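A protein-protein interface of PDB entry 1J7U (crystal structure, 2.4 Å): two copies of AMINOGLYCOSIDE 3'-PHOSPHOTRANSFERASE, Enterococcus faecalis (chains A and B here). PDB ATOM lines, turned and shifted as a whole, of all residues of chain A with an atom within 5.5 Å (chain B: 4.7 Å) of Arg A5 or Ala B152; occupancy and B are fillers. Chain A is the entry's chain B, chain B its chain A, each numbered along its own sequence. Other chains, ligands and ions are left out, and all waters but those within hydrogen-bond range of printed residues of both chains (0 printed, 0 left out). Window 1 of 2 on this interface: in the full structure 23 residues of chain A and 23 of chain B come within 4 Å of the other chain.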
ATOM      1  N   LYS A   3      23.247  35.913  -8.435  1.00  0.00           N
ATOM      2  CA  LYS A   3      23.171  34.499  -8.094  1.00  0.00           C
ATOM      3  C   LYS A   3      21.740  33.978  -8.237  1.00  0.00           C
ATOM      4  O   LYS A   3      20.804  34.546  -7.672  1.00  0.00           O
ATOM      5  CB  LYS A   3      23.676  34.247  -6.673  1.00  0.00           C
ATOM      6  CG  LYS A   3      23.712  32.769  -6.311  1.00  0.00           C
ATOM      7  CD  LYS A   3      24.263  32.515  -4.915  1.00  0.00           C
ATOM      8  CE  LYS A   3      24.469  31.023  -4.700  1.00  0.00           C
ATOM      9  NZ  LYS A   3      24.847  30.696  -3.301  1.00  0.00           N
ATOM     10  N   MET A   4      21.593  32.909  -9.017  1.00  0.00           N
ATOM     11  CA  MET A   4      20.304  32.262  -9.272  1.00  0.00           C
ATOM     12  C   MET A   4      20.523  30.779  -9.559  1.00  0.00           C
ATOM     13  O   MET A   4      21.640  30.360  -9.869  1.00  0.00           O
ATOM     14  CB  MET A   4      19.601  32.891 -10.481  1.00  0.00           C
ATOM     15  CG  MET A   4      19.013  34.272 -10.252  1.00  0.00           C
ATOM     16  SD  MET A   4      17.320  34.372 -10.866  1.00  0.00           S
ATOM     17  CE  MET A   4      17.574  34.120 -12.617  1.00  0.00           C
ATOM     18  N   ARG A   5      19.453  29.992  -9.466  1.00  0.00           N
ATOM     19  CA  ARG A   5      19.527  28.558  -9.731  1.00  0.00           C
ATOM     20  C   ARG A   5      19.400  28.209 -11.218  1.00  0.00           C
ATOM     21  O   ARG A   5      19.763  27.109 -11.632  1.00  0.00           O
ATOM     22  CB  ARG A   5      18.467  27.815  -8.923  1.00  0.00           C
ATOM     23  CG  ARG A   5      18.744  27.800  -7.434  1.00  0.00           C
ATOM     24  CD  ARG A   5      17.663  27.070  -6.683  1.00  0.00           C
ATOM     25  NE  ARG A   5      18.004  26.907  -5.274  1.00  0.00           N
ATOM     26  CZ  ARG A   5      17.168  26.428  -4.354  1.00  0.00           C
ATOM     27  NH1 ARG A   5      15.941  26.071  -4.699  1.00  0.00           N
ATOM     28  NH2 ARG A   5      17.569  26.269  -3.099  1.00  0.00           N
ATOM     29  N   ILE A   6      18.874  29.139 -12.012  1.00  0.00           N
ATOM     30  CA  ILE A   6      18.723  28.926 -13.452  1.00  0.00           C
ATOM     31  C   ILE A   6      19.426  30.057 -14.193  1.00  0.00           C
ATOM     32  O   ILE A   6      19.472  31.185 -13.707  1.00  0.00           O
ATOM     33  CB  ILE A   6      17.232  28.838 -13.889  1.00  0.00           C
ATOM     34  CG1 ILE A   6      16.507  30.161 -13.642  1.00  0.00           C
ATOM     35  CG2 ILE A   6      16.524  27.704 -13.132  1.00  0.00           C
ATOM     36  CD1 ILE A   6      15.062  30.153 -14.102  1.00  0.00           C
ATOM     37  N   SER A   7      19.995  29.749 -15.354  1.00  0.00           N
ATOM     38  CA  SER A   7      20.719  30.742 -16.154  1.00  0.00           C
ATOM     39  C   SER A   7      19.807  31.809 -16.772  1.00  0.00           C
ATOM     40  O   SER A   7      18.582  31.652 -16.804  1.00  0.00           O
ATOM     41  CB  SER A   7      21.483  30.041 -17.277  1.00  0.00           C
ATOM     42  OG  SER A   7      20.586  29.563 -18.267  1.00  0.00           O
ATOM     43  N   LYS A  30      13.438  18.996  -7.826  1.00  0.00           N
ATOM     44  CA  LYS A  30      12.496  20.099  -7.811  1.00  0.00           C
ATOM     45  C   LYS A  30      11.739  19.994  -9.128  1.00  0.00           C
ATOM     46  O   LYS A  30      12.349  20.032 -10.194  1.00  0.00           O
ATOM     47  CB  LYS A  30      13.245  21.435  -7.750  1.00  0.00           C
ATOM     48  CG  LYS A  30      14.041  21.647  -6.472  1.00  0.00           C
ATOM     49  CD  LYS A  30      13.128  22.028  -5.329  1.00  0.00           C
ATOM     50  CE  LYS A  30      13.863  22.015  -4.001  1.00  0.00           C
ATOM     51  NZ  LYS A  30      14.173  20.623  -3.551  1.00  0.00           N
ATOM     52  N   TYR A  32       8.622  21.531 -11.510  1.00  0.00           N
ATOM     53  CA  TYR A  32       7.752  22.676 -11.739  1.00  0.00           C
ATOM     54  C   TYR A  32       6.972  22.563 -13.031  1.00  0.00           C
ATOM     55  O   TYR A  32       7.542  22.331 -14.098  1.00  0.00           O
ATOM     56  CB  TYR A  32       8.559  23.982 -11.790  1.00  0.00           C
ATOM     57  CG  TYR A  32       9.431  24.220 -10.591  1.00  0.00           C
ATOM     58  CD1 TYR A  32      10.790  23.904 -10.625  1.00  0.00           C
ATOM     59  CD2 TYR A  32       8.898  24.728  -9.411  1.00  0.00           C
ATOM     60  CE1 TYR A  32      11.596  24.082  -9.509  1.00  0.00           C
ATOM     61  CE2 TYR A  32       9.696  24.915  -8.290  1.00  0.00           C
ATOM     62  CZ  TYR A  32      11.046  24.587  -8.344  1.00  0.00           C
ATOM     63  OH  TYR A  32      11.843  24.749  -7.229  1.00  0.00           O
ATOM     64  N   MET A  45      14.767  19.904 -11.509  1.00  0.00           N
ATOM     65  CA  MET A  45      16.094  20.326 -11.054  1.00  0.00           C
ATOM     66  C   MET A  45      16.646  19.526  -9.877  1.00  0.00           C
ATOM     67  O   MET A  45      15.918  19.213  -8.932  1.00  0.00           O
ATOM     68  CB  MET A  45      16.040  21.802 -10.614  1.00  0.00           C
ATOM     69  CG  MET A  45      15.460  22.767 -11.622  1.00  0.00           C
ATOM     70  SD  MET A  45      15.012  24.334 -10.843  1.00  0.00           S
ATOM     71  CE  MET A  45      16.639  24.907 -10.284  1.00  0.00           C
ATOM     72  N   GLU A  80      20.959  22.184 -18.669  1.00  0.00           N
ATOM     73  CA  GLU A  80      22.118  22.952 -18.243  1.00  0.00           C
ATOM     74  C   GLU A  80      22.614  22.581 -16.861  1.00  0.00           C
ATOM     75  O   GLU A  80      21.883  22.031 -16.026  1.00  0.00           O
ATOM     76  CB  GLU A  80      21.796  24.455 -18.230  1.00  0.00           C
ATOM     77  CG  GLU A  80      20.932  24.897 -17.043  1.00  0.00           C
ATOM     78  CD  GLU A  80      20.496  26.351 -17.128  1.00  0.00           C
ATOM     79  OE1 GLU A  80      20.050  26.902 -16.095  1.00  0.00           O
ATOM     80  OE2 GLU A  80      20.597  26.944 -18.226  1.00  0.00           O
ATOM     81  N   HIS A  82      24.072  24.589 -13.868  1.00  0.00           N
ATOM     82  CA  HIS A  82      24.165  25.980 -13.454  1.00  0.00           C
ATOM     83  C   HIS A  82      24.346  26.169 -11.966  1.00  0.00           C
ATOM     84  O   HIS A  82      23.457  25.845 -11.173  1.00  0.00           O
ATOM     85  CB  HIS A  82      22.946  26.783 -13.931  1.00  0.00           C
ATOM     86  CG  HIS A  82      23.033  28.242 -13.608  1.00  0.00           C
ATOM     87  ND1 HIS A  82      23.671  29.147 -14.425  1.00  0.00           N
ATOM     88  CD2 HIS A  82      22.618  28.941 -12.524  1.00  0.00           C
ATOM     89  CE1 HIS A  82      23.654  30.340 -13.857  1.00  0.00           C
ATOM     90  NE2 HIS A  82      23.021  30.243 -12.703  1.00  0.00           N
ATOM     91  N   TRP A  85      23.502  23.349  -9.801  1.00  0.00           N
ATOM     92  CA  TRP A  85      22.250  22.717 -10.210  1.00  0.00           C
ATOM     93  C   TRP A  85      22.267  22.083 -11.601  1.00  0.00           C
ATOM     94  O   TRP A  85      23.047  22.474 -12.465  1.00  0.00           O
ATOM     95  CB  TRP A  85      21.108  23.739 -10.148  1.00  0.00           C
ATOM     96  CG  TRP A  85      20.731  24.127  -8.754  1.00  0.00           C
ATOM     97  CD1 TRP A  85      21.294  25.114  -7.993  1.00  0.00           C
ATOM     98  CD2 TRP A  85      19.744  23.498  -7.932  1.00  0.00           C
ATOM     99  NE1 TRP A  85      20.723  25.133  -6.745  1.00  0.00           N
ATOM    100  CE2 TRP A  85      19.768  24.152  -6.678  1.00  0.00           C
ATOM    101  CE3 TRP A  85      18.845  22.441  -8.129  1.00  0.00           C
ATOM    102  CZ2 TRP A  85      18.925  23.781  -5.624  1.00  0.00           C
ATOM    103  CZ3 TRP A  85      18.006  22.073  -7.083  1.00  0.00           C
ATOM    104  CH2 TRP A  85      18.051  22.742  -5.844  1.00  0.00           C
ATOM    105  N   ASN A  87      19.573  21.394 -14.443  1.00  0.00           N
ATOM    106  CA  ASN A  87      18.218  21.756 -14.844  1.00  0.00           C
ATOM    107  C   ASN A  87      17.760  21.174 -16.172  1.00  0.00           C
ATOM    108  O   ASN A  87      18.466  21.254 -17.175  1.00  0.00           O
ATOM    109  CB  ASN A  87      18.104  23.283 -14.883  1.00  0.00           C
ATOM    110  CG  ASN A  87      18.620  23.933 -13.614  1.00  0.00           C
ATOM    111  OD1 ASN A  87      18.513  23.366 -12.525  1.00  0.00           O
ATOM    112  ND2 ASN A  87      19.196  25.122 -13.747  1.00  0.00           N
ATOM    113  N   LEU B 146      21.547  32.515   4.269  1.00  0.00           N
ATOM    114  CA  LEU B 146      20.727  31.594   3.487  1.00  0.00           C
ATOM    115  C   LEU B 146      20.913  31.757   1.990  1.00  0.00           C
ATOM    116  O   LEU B 146      20.977  30.759   1.262  1.00  0.00           O
ATOM    117  CB  LEU B 146      19.247  31.753   3.841  1.00  0.00           C
ATOM    118  CG  LEU B 146      18.856  31.486   5.300  1.00  0.00           C
ATOM    119  CD1 LEU B 146      17.407  31.900   5.536  1.00  0.00           C
ATOM    120  CD2 LEU B 146      19.074  30.027   5.651  1.00  0.00           C
ATOM    121  N   LEU B 147      20.981  33.009   1.535  1.00  0.00           N
ATOM    122  CA  LEU B 147      21.168  33.304   0.119  1.00  0.00           C
ATOM    123  C   LEU B 147      22.556  32.874  -0.322  1.00  0.00           C
ATOM    124  O   LEU B 147      22.711  32.256  -1.370  1.00  0.00           O
ATOM    125  CB  LEU B 147      20.990  34.798  -0.170  1.00  0.00           C
ATOM    126  CG  LEU B 147      19.568  35.351  -0.129  1.00  0.00           C
ATOM    127  CD1 LEU B 147      19.574  36.853  -0.374  1.00  0.00           C
ATOM    128  CD2 LEU B 147      18.715  34.640  -1.157  1.00  0.00           C
ATOM    129  N   ASP B 150      22.639  29.157  -0.671  1.00  0.00           N
ATOM    130  CA  ASP B 150      21.568  28.599  -1.502  1.00  0.00           C
ATOM    131  C   ASP B 150      20.559  27.774  -0.702  1.00  0.00           C
ATOM    132  O   ASP B 150      20.096  26.724  -1.149  1.00  0.00           O
ATOM    133  CB  ASP B 150      22.168  27.765  -2.650  1.00  0.00           C
ATOM    134  CG  ASP B 150      21.144  27.411  -3.723  1.00  0.00           C
ATOM    135  OD1 ASP B 150      20.207  28.201  -3.962  1.00  0.00           O
ATOM    136  OD2 ASP B 150      21.276  26.331  -4.333  1.00  0.00           O
ATOM    137  N   LEU B 151      20.198  28.281   0.472  1.00  0.00           N
ATOM    138  CA  LEU B 151      19.251  27.605   1.351  1.00  0.00           C
ATOM    139  C   LEU B 151      17.945  28.370   1.493  1.00  0.00           C
ATOM    140  O   LEU B 151      17.054  27.942   2.218  1.00  0.00           O
ATOM    141  CB  LEU B 151      19.877  27.401   2.729  1.00  0.00           C
ATOM    142  CG  LEU B 151      21.156  26.559   2.731  1.00  0.00           C
ATOM    143  CD1 LEU B 151      21.801  26.569   4.111  1.00  0.00           C
ATOM    144  CD2 LEU B 151      20.825  25.140   2.275  1.00  0.00           C
ATOM    145  N   ALA B 152      17.849  29.513   0.817  1.00  0.00           N
ATOM    146  CA  ALA B 152      16.644  30.329   0.872  1.00  0.00           C
ATOM    147  C   ALA B 152      15.568  29.765  -0.045  1.00  0.00           C
ATOM    148  O   ALA B 152      15.846  28.935  -0.911  1.00  0.00           O
ATOM    149  CB  ALA B 152      16.955  31.767   0.504  1.00  0.00           C
ATOM    150  N   ASP B 153      14.338  30.222   0.154  1.00  0.00           N
ATOM    151  CA  ASP B 153      13.215  29.755  -0.643  1.00  0.00           C
ATOM    152  C   ASP B 153      13.039  30.537  -1.937  1.00  0.00           C
ATOM    153  O   ASP B 153      12.614  31.690  -1.924  1.00  0.00           O
ATOM    154  CB  ASP B 153      11.931  29.814   0.181  1.00  0.00           C
ATOM    155  CG  ASP B 153      10.791  29.074  -0.475  1.00  0.00           C
ATOM    156  OD1 ASP B 153       9.792  29.726  -0.841  1.00  0.00           O
ATOM    157  OD2 ASP B 153      10.902  27.838  -0.625  1.00  0.00           O
ATOM    158  N   VAL B 154      13.379  29.901  -3.053  1.00  0.00           N
ATOM    159  CA  VAL B 154      13.245  30.532  -4.359  1.00  0.00           C
ATOM    160  C   VAL B 154      11.881  30.192  -4.968  1.00  0.00           C
ATOM    161  O   VAL B 154      11.745  29.246  -5.753  1.00  0.00           O
ATOM    162  CB  VAL B 154      14.412  30.135  -5.314  1.00  0.00           C
ATOM    163  N   LEU B 263      11.556  35.470   0.537  1.00  0.00           N
ATOM    164  CA  LEU B 263      12.737  34.613   0.471  1.00  0.00           C
ATOM    165  C   LEU B 263      12.839  33.581   1.601  1.00  0.00           C
ATOM    166  O   LEU B 263      13.888  32.983   1.799  1.00  0.00           O
ATOM    167  CB  LEU B 263      14.012  35.468   0.408  1.00  0.00           C
ATOM    168  CG  LEU B 263      14.131  36.435  -0.785  1.00  0.00           C
ATOM    169  CD1 LEU B 263      15.173  37.527  -0.516  1.00  0.00           C
ATOM    170  CD2 LEU B 263      14.468  35.666  -2.056  1.00  0.00           C
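The indole nitrogen (NE1) of Trp A85 sits at hydrogen-bond distance from the side-chain carboxylate (OD2) of Asp B150 (2.7 Å).
The backbone carbonyl oxygen (O) of Leu B147 lies within hydrogen-bond range of the side-chain amino group (NZ) of Lys A3 (3.3 Å).
The side-chain carboxylate of Asp B150 is in salt-bridge range of the guanidinium group of Arg A5.
Of chain B, only Asp B150 (2.9 Å) and Ala B152 (3.9 Å) come within 4 Å of Arg A5.
Ala B152 touches just one residue of chain A: Arg A5 (3.9 Å).
Of the printed residues of chain A, Leu B147 touches Lys A3.
Of the printed residues of chain B, Lys A3 touches Leu B147 (3.3 Å) and Asp B150 (3.8 Å).
Lys A30 touches none of the printed residues of chain B.
Ser A7 touches none of the printed residues of chain B.
The nearest printed residue of chain A that does not touch Ala B152 is Trp A85 (7.6 Å).
The nearest printed residue of chain B that does not touch Trp A85 is Ala B152 (7.6 Å).
No position is printed for both chains.
Of the 5 pairs that touch across the chains among the printed residues, none has its exchanged pair printed and touching as well.
Among the printed residues, pairs that only touch across the chains: Lys A3 with Asp B150 (3.8 Å) and Arg A5 with Ala B152 (3.9 Å).
Printed residues of chain B that touch a printed residue of chain A: Leu B147, Asp B150 and Ala B152.
Among the printed residues, Asp or Glu carboxylates within 4 Å of a Lys or Arg side-chain nitrogen of the other chain: Arg A5 with Asp B150.
The backbone carbonyl oxygen of Arg A5 sits at hydrogen-bond distance from the side-chain amide nitrogen of Asn A87 (3.0 Å).
O of Leu B146 is in hydrogen-bond range of N of Ala B152.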
